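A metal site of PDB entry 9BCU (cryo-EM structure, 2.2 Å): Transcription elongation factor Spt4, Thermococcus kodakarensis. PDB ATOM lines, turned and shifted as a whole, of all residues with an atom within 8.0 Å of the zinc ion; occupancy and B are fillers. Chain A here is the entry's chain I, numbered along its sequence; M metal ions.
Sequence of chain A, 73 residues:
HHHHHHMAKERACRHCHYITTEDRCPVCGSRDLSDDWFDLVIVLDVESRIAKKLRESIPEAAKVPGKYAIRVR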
ATOM      1  N   ALA A  12     -25.577  -5.405 -23.064  1.00  0.00           N
ATOM      2  CA  ALA A  12     -24.849  -4.331 -22.413  1.00  0.00           C
ATOM      3  C   ALA A  12     -23.545  -4.848 -21.825  1.00  0.00           C
ATOM      4  O   ALA A  12     -23.476  -5.971 -21.331  1.00  0.00           O
ATOM      5  CB  ALA A  12     -25.690  -3.691 -21.304  1.00  0.00           C
ATOM      6  N   CYS A  13     -22.510  -4.017 -21.900  1.00  0.00           N
ATOM      7  CA  CYS A  13     -21.204  -4.399 -21.374  1.00  0.00           C
ATOM      8  C   CYS A  13     -21.210  -4.395 -19.859  1.00  0.00           C
ATOM      9  O   CYS A  13     -21.878  -3.587 -19.218  1.00  0.00           O
ATOM     10  CB  CYS A  13     -20.124  -3.442 -21.899  1.00  0.00           C
ATOM     11  SG  CYS A  13     -18.460  -3.811 -21.322  1.00  0.00           S
ATOM     12  N   ARG A  14     -20.456  -5.337 -19.272  1.00  0.00           N
ATOM     13  CA  ARG A  14     -20.356  -5.412 -17.818  1.00  0.00           C
ATOM     14  C   ARG A  14     -19.362  -4.405 -17.243  1.00  0.00           C
ATOM     15  O   ARG A  14     -19.381  -4.158 -16.036  1.00  0.00           O
ATOM     16  CB  ARG A  14     -19.962  -6.824 -17.383  1.00  0.00           C
ATOM     17  CG  ARG A  14     -20.882  -7.915 -17.908  1.00  0.00           C
ATOM     18  CD  ARG A  14     -20.905  -9.100 -16.949  1.00  0.00           C
ATOM     19  NE  ARG A  14     -22.133  -9.885 -17.048  1.00  0.00           N
ATOM     20  CZ  ARG A  14     -22.458 -10.667 -18.068  1.00  0.00           C
ATOM     21  NH1 ARG A  14     -21.664 -10.811 -19.107  1.00  0.00           N
ATOM     22  NH2 ARG A  14     -23.615 -11.322 -18.035  1.00  0.00           N
ATOM     23  N   HIS A  15     -18.490  -3.829 -18.074  1.00  0.00           N
ATOM     24  CA  HIS A  15     -17.461  -2.906 -17.609  1.00  0.00           C
ATOM     25  C   HIS A  15     -17.903  -1.450 -17.741  1.00  0.00           C
ATOM     26  O   HIS A  15     -17.965  -0.725 -16.733  1.00  0.00           O
ATOM     27  CB  HIS A  15     -16.165  -3.140 -18.393  1.00  0.00           C
ATOM     28  CG  HIS A  15     -15.033  -2.244 -17.969  1.00  0.00           C
ATOM     29  ND1 HIS A  15     -14.359  -1.437 -18.854  1.00  0.00           N
ATOM     30  CD2 HIS A  15     -14.470  -2.032 -16.763  1.00  0.00           C
ATOM     31  CE1 HIS A  15     -13.425  -0.763 -18.207  1.00  0.00           C
ATOM     32  NE2 HIS A  15     -13.474  -1.108 -16.931  1.00  0.00           N
ATOM     33  N   CYS A  16     -18.201  -0.994 -18.959  1.00  0.00           N
ATOM     34  CA  CYS A  16     -18.573   0.389 -19.199  1.00  0.00           C
ATOM     35  C   CYS A  16     -20.071   0.601 -19.318  1.00  0.00           C
ATOM     36  O   CYS A  16     -20.508   1.734 -19.554  1.00  0.00           O
ATOM     37  CB  CYS A  16     -17.879   0.895 -20.473  1.00  0.00           C
ATOM     38  SG  CYS A  16     -18.216  -0.091 -21.941  1.00  0.00           S
ATOM     39  N   HIS A  17     -20.871  -0.455 -19.150  1.00  0.00           N
ATOM     40  CA  HIS A  17     -22.334  -0.386 -19.207  1.00  0.00           C
ATOM     41  C   HIS A  17     -22.818   0.203 -20.527  1.00  0.00           C
ATOM     42  O   HIS A  17     -23.731   1.034 -20.558  1.00  0.00           O
ATOM     43  CB  HIS A  17     -22.897   0.411 -18.015  1.00  0.00           C
ATOM     44  CG  HIS A  17     -22.799  -0.309 -16.712  1.00  0.00           C
ATOM     45  ND1 HIS A  17     -23.813  -0.300 -15.777  1.00  0.00           N
ATOM     46  CD2 HIS A  17     -21.813  -1.063 -16.174  1.00  0.00           C
ATOM     47  CE1 HIS A  17     -23.449  -1.016 -14.728  1.00  0.00           C
ATOM     48  NE2 HIS A  17     -22.235  -1.488 -14.939  1.00  0.00           N
ATOM     49  N   TYR A  18     -22.219  -0.229 -21.629  1.00  0.00           N
ATOM     50  CA  TYR A  18     -22.545   0.259 -22.964  1.00  0.00           C
ATOM     51  C   TYR A  18     -23.320  -0.816 -23.719  1.00  0.00           C
ATOM     52  O   TYR A  18     -22.909  -1.978 -23.740  1.00  0.00           O
ATOM     53  CB  TYR A  18     -21.272   0.641 -23.726  1.00  0.00           C
ATOM     54  CG  TYR A  18     -21.507   1.433 -24.995  1.00  0.00           C
ATOM     55  CD1 TYR A  18     -21.845   0.809 -26.184  1.00  0.00           C
ATOM     56  CD2 TYR A  18     -21.392   2.820 -24.999  1.00  0.00           C
ATOM     57  CE1 TYR A  18     -22.061   1.533 -27.342  1.00  0.00           C
ATOM     58  CE2 TYR A  18     -21.610   3.549 -26.149  1.00  0.00           C
ATOM     59  CZ  TYR A  18     -21.940   2.894 -27.319  1.00  0.00           C
ATOM     60  OH  TYR A  18     -22.158   3.623 -28.469  1.00  0.00           O
ATOM     61  N   ILE A  19     -24.434  -0.418 -24.326  1.00  0.00           N
ATOM     62  CA  ILE A  19     -25.262  -1.322 -25.104  1.00  0.00           C
ATOM     63  C   ILE A  19     -24.788  -1.288 -26.556  1.00  0.00           C
ATOM     64  O   ILE A  19     -24.779  -0.223 -27.174  1.00  0.00           O
ATOM     65  CB  ILE A  19     -26.749  -0.963 -24.998  1.00  0.00           C
ATOM     66  CG1 ILE A  19     -27.282  -1.285 -23.601  1.00  0.00           C
ATOM     67  CG2 ILE A  19     -27.559  -1.688 -26.054  1.00  0.00           C
ATOM     68  CD1 ILE A  19     -27.507  -0.075 -22.730  1.00  0.00           C
ATOM     69  N   THR A  20     -24.416  -2.446 -27.086  1.00  0.00           N
ATOM     70  CA  THR A  20     -23.959  -2.557 -28.463  1.00  0.00           C
ATOM     71  C   THR A  20     -24.599  -3.773 -29.112  1.00  0.00           C
ATOM     72  O   THR A  20     -24.991  -4.731 -28.429  1.00  0.00           O
ATOM     73  CB  THR A  20     -22.426  -2.642 -28.556  1.00  0.00           C
ATOM     74  OG1 THR A  20     -22.036  -2.745 -29.930  1.00  0.00           O
ATOM     75  CG2 THR A  20     -21.912  -3.835 -27.783  1.00  0.00           C
ATOM     76  N   ARG A  24     -17.889  -7.044 -30.468  1.00  0.00           N
ATOM     77  CA  ARG A  24     -16.832  -6.130 -30.037  1.00  0.00           C
ATOM     78  C   ARG A  24     -17.420  -4.957 -29.262  1.00  0.00           C
ATOM     79  O   ARG A  24     -18.501  -4.465 -29.565  1.00  0.00           O
ATOM     80  CB  ARG A  24     -16.056  -5.613 -31.252  1.00  0.00           C
ATOM     81  CG  ARG A  24     -15.140  -6.647 -31.888  1.00  0.00           C
ATOM     82  CD  ARG A  24     -14.274  -6.032 -32.973  1.00  0.00           C
ATOM     83  NE  ARG A  24     -13.413  -7.014 -33.615  1.00  0.00           N
ATOM     84  CZ  ARG A  24     -12.659  -6.768 -34.677  1.00  0.00           C
ATOM     85  NH1 ARG A  24     -12.626  -5.566 -35.237  1.00  0.00           N
ATOM     86  NH2 ARG A  24     -11.908  -7.744 -35.185  1.00  0.00           N
ATOM     87  N   CYS A  25     -16.686  -4.526 -28.239  1.00  0.00           N
ATOM     88  CA  CYS A  25     -17.089  -3.379 -27.432  1.00  0.00           C
ATOM     89  C   CYS A  25     -16.357  -2.144 -27.920  1.00  0.00           C
ATOM     90  O   CYS A  25     -15.121  -2.087 -27.797  1.00  0.00           O
ATOM     91  CB  CYS A  25     -16.799  -3.630 -25.955  1.00  0.00           C
ATOM     92  SG  CYS A  25     -17.604  -2.473 -24.816  1.00  0.00           S
ATOM     93  N   PRO A  26     -17.038  -1.145 -28.463  1.00  0.00           N
ATOM     94  CA  PRO A  26     -16.356   0.036 -29.003  1.00  0.00           C
ATOM     95  C   PRO A  26     -15.847   1.016 -27.968  1.00  0.00           C
ATOM     96  O   PRO A  26     -15.398   2.106 -28.338  1.00  0.00           O
ATOM     97  CB  PRO A  26     -17.449   0.700 -29.877  1.00  0.00           C
ATOM     98  CG  PRO A  26     -18.592  -0.278 -29.921  1.00  0.00           C
ATOM     99  CD  PRO A  26     -18.494  -1.092 -28.684  1.00  0.00           C
ATOM    100  N   VAL A  27     -15.897   0.676 -26.683  1.00  0.00           N
ATOM    101  CA  VAL A  27     -15.425   1.547 -25.609  1.00  0.00           C
ATOM    102  C   VAL A  27     -14.194   0.950 -24.914  1.00  0.00           C
ATOM    103  O   VAL A  27     -13.132   1.574 -24.882  1.00  0.00           O
ATOM    104  CB  VAL A  27     -16.544   1.844 -24.587  1.00  0.00           C
ATOM    105  CG1 VAL A  27     -16.123   2.943 -23.624  1.00  0.00           C
ATOM    106  CG2 VAL A  27     -17.832   2.231 -25.309  1.00  0.00           C
ATOM    107  N   CYS A  28     -14.322  -0.247 -24.355  1.00  0.00           N
ATOM    108  CA  CYS A  28     -13.240  -0.895 -23.644  1.00  0.00           C
ATOM    109  C   CYS A  28     -12.799  -2.217 -24.256  1.00  0.00           C
ATOM    110  O   CYS A  28     -11.801  -2.791 -23.788  1.00  0.00           O
ATOM    111  CB  CYS A  28     -13.621  -1.129 -22.179  1.00  0.00           C
ATOM    112  SG  CYS A  28     -15.074  -2.191 -21.948  1.00  0.00           S
ATOM    113  N   GLY A  29     -13.491  -2.714 -25.269  1.00  0.00           N
ATOM    114  CA  GLY A  29     -13.142  -3.989 -25.880  1.00  0.00           C
ATOM    115  C   GLY A  29     -13.327  -5.191 -24.973  1.00  0.00           C
ATOM    116  O   GLY A  29     -12.503  -6.110 -24.996  1.00  0.00           O
ATOM    117  N   SER A  30     -14.395  -5.203 -24.178  1.00  0.00           N
ATOM    118  CA  SER A  30     -14.682  -6.311 -23.286  1.00  0.00           C
ATOM    119  C   SER A  30     -15.477  -7.386 -24.010  1.00  0.00           C
ATOM    120  O   SER A  30     -16.329  -7.103 -24.855  1.00  0.00           O
ATOM    121  CB  SER A  30     -15.451  -5.832 -22.062  1.00  0.00           C
ATOM    122  OG  SER A  30     -14.573  -5.539 -20.989  1.00  0.00           O
ATOM    123  N   ARG A  31     -15.186  -8.644 -23.671  1.00  0.00           N
ATOM    124  CA  ARG A  31     -15.831  -9.792 -24.299  1.00  0.00           C
ATOM    125  C   ARG A  31     -16.971 -10.363 -23.462  1.00  0.00           C
ATOM    126  O   ARG A  31     -17.562 -11.371 -23.852  1.00  0.00           O
ATOM    127  CB  ARG A  31     -14.794 -10.883 -24.575  1.00  0.00           C
ATOM    128  CG  ARG A  31     -13.712 -10.474 -25.558  1.00  0.00           C
ATOM    129  CD  ARG A  31     -12.666 -11.566 -25.716  1.00  0.00           C
ATOM    130  NE  ARG A  31     -11.575 -11.144 -26.588  1.00  0.00           N
ATOM    131  CZ  ARG A  31     -10.445 -11.819 -26.755  1.00  0.00           C
ATOM    132  NH1 ARG A  31     -10.217 -12.953 -26.126  1.00  0.00           N
ATOM    133  NH2 ARG A  31      -9.518 -11.341 -27.590  1.00  0.00           N
ATOM    134  N   ASP A  32     -17.287  -9.750 -22.324  1.00  0.00           N
ATOM    135  CA  ASP A  32     -18.367 -10.211 -21.451  1.00  0.00           C
ATOM    136  C   ASP A  32     -19.482  -9.172 -21.489  1.00  0.00           C
ATOM    137  O   ASP A  32     -19.391  -8.128 -20.849  1.00  0.00           O
ATOM    138  CB  ASP A  32     -17.854 -10.438 -20.030  1.00  0.00           C
ATOM    139  CG  ASP A  32     -16.830  -9.411 -19.610  1.00  0.00           C
ATOM    140  OD1 ASP A  32     -16.512  -8.507 -20.419  1.00  0.00           O
ATOM    141  OD2 ASP A  32     -16.331  -9.499 -18.464  1.00  0.00           O
ATOM    142  N   LEU A  33     -20.536  -9.477 -22.236  1.00  0.00           N
ATOM    143  CA  LEU A  33     -21.689  -8.602 -22.368  1.00  0.00           C
ATOM    144  C   LEU A  33     -22.930  -9.313 -21.826  1.00  0.00           C
ATOM    145  O   LEU A  33     -23.081 -10.521 -21.996  1.00  0.00           O
ATOM    146  CB  LEU A  33     -21.930  -8.177 -23.822  1.00  0.00           C
ATOM    147  CG  LEU A  33     -20.749  -7.660 -24.656  1.00  0.00           C
ATOM    148  CD1 LEU A  33     -21.251  -6.991 -25.919  1.00  0.00           C
ATOM    149  CD2 LEU A  33     -19.872  -6.686 -23.870  1.00  0.00           C
ATOM    150  N   GLU A  60     -16.511   4.058 -15.460  1.00  0.00           N
ATOM    151  CA  GLU A  60     -16.331   3.798 -16.890  1.00  0.00           C
ATOM    152  C   GLU A  60     -17.497   4.298 -17.738  1.00  0.00           C
ATOM    153  O   GLU A  60     -17.385   4.283 -18.967  1.00  0.00           O
ATOM    154  CB  GLU A  60     -16.141   2.297 -17.126  1.00  0.00           C
ATOM    155  N   TYR A  68     -26.566   3.735 -22.567  1.00  0.00           N
ATOM    156  CA  TYR A  68     -25.957   3.254 -21.334  1.00  0.00           C
ATOM    157  C   TYR A  68     -27.009   2.576 -20.477  1.00  0.00           C
ATOM    158  O   TYR A  68     -28.219   2.796 -20.639  1.00  0.00           O
ATOM    159  CB  TYR A  68     -25.295   4.405 -20.554  1.00  0.00           C
ATOM    160  CG  TYR A  68     -23.976   4.860 -21.125  1.00  0.00           C
ATOM    161  CD1 TYR A  68     -22.829   4.082 -20.978  1.00  0.00           C
ATOM    162  CD2 TYR A  68     -23.872   6.055 -21.804  1.00  0.00           C
ATOM    163  CE1 TYR A  68     -21.621   4.488 -21.501  1.00  0.00           C
ATOM    164  CE2 TYR A  68     -22.663   6.472 -22.334  1.00  0.00           C
ATOM    165  CZ  TYR A  68     -21.546   5.684 -22.176  1.00  0.00           C
ATOM    166  OH  TYR A  68     -20.338   6.102 -22.706  1.00  0.00           O
HETATM  167 ZN    ZN M   1     -17.333  -2.159 -22.525  1.00  0.00          ZN
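N of Cys 13 sits at hydrogen-bond distance from O of Tyr 18. OG of Ser 30 lies close to SG of Cys 28 (3.5 Å). The side-chain sulfur of Cys 13 lies close to the backbone NH of His 15, at 3.2 Å. The side-chain sulfur (SG) of Cys 28 sits close to a ring nitrogen (ND1) of His 15 (3.3 Å).
Four residues have an atom within 4 Å of the zinc ion: Cys 13, Cys 16, Cys 25 and Cys 28. The nearest printed residue that does not touch the zinc ion is Ser 30 (4.2 Å).
The zinc ion is bound by the side-chain sulfur (SG) of Cys 16. The side-chain sulfur (SG) of Cys 25 is bound to the zinc ion, at 2.3 Å. SG of Cys 28 binds the zinc ion, 2.3 Å away. SG of Cys 13 is bound to the zinc ion (2.3 Å). The zinc ion has four donor atoms within binding distance.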
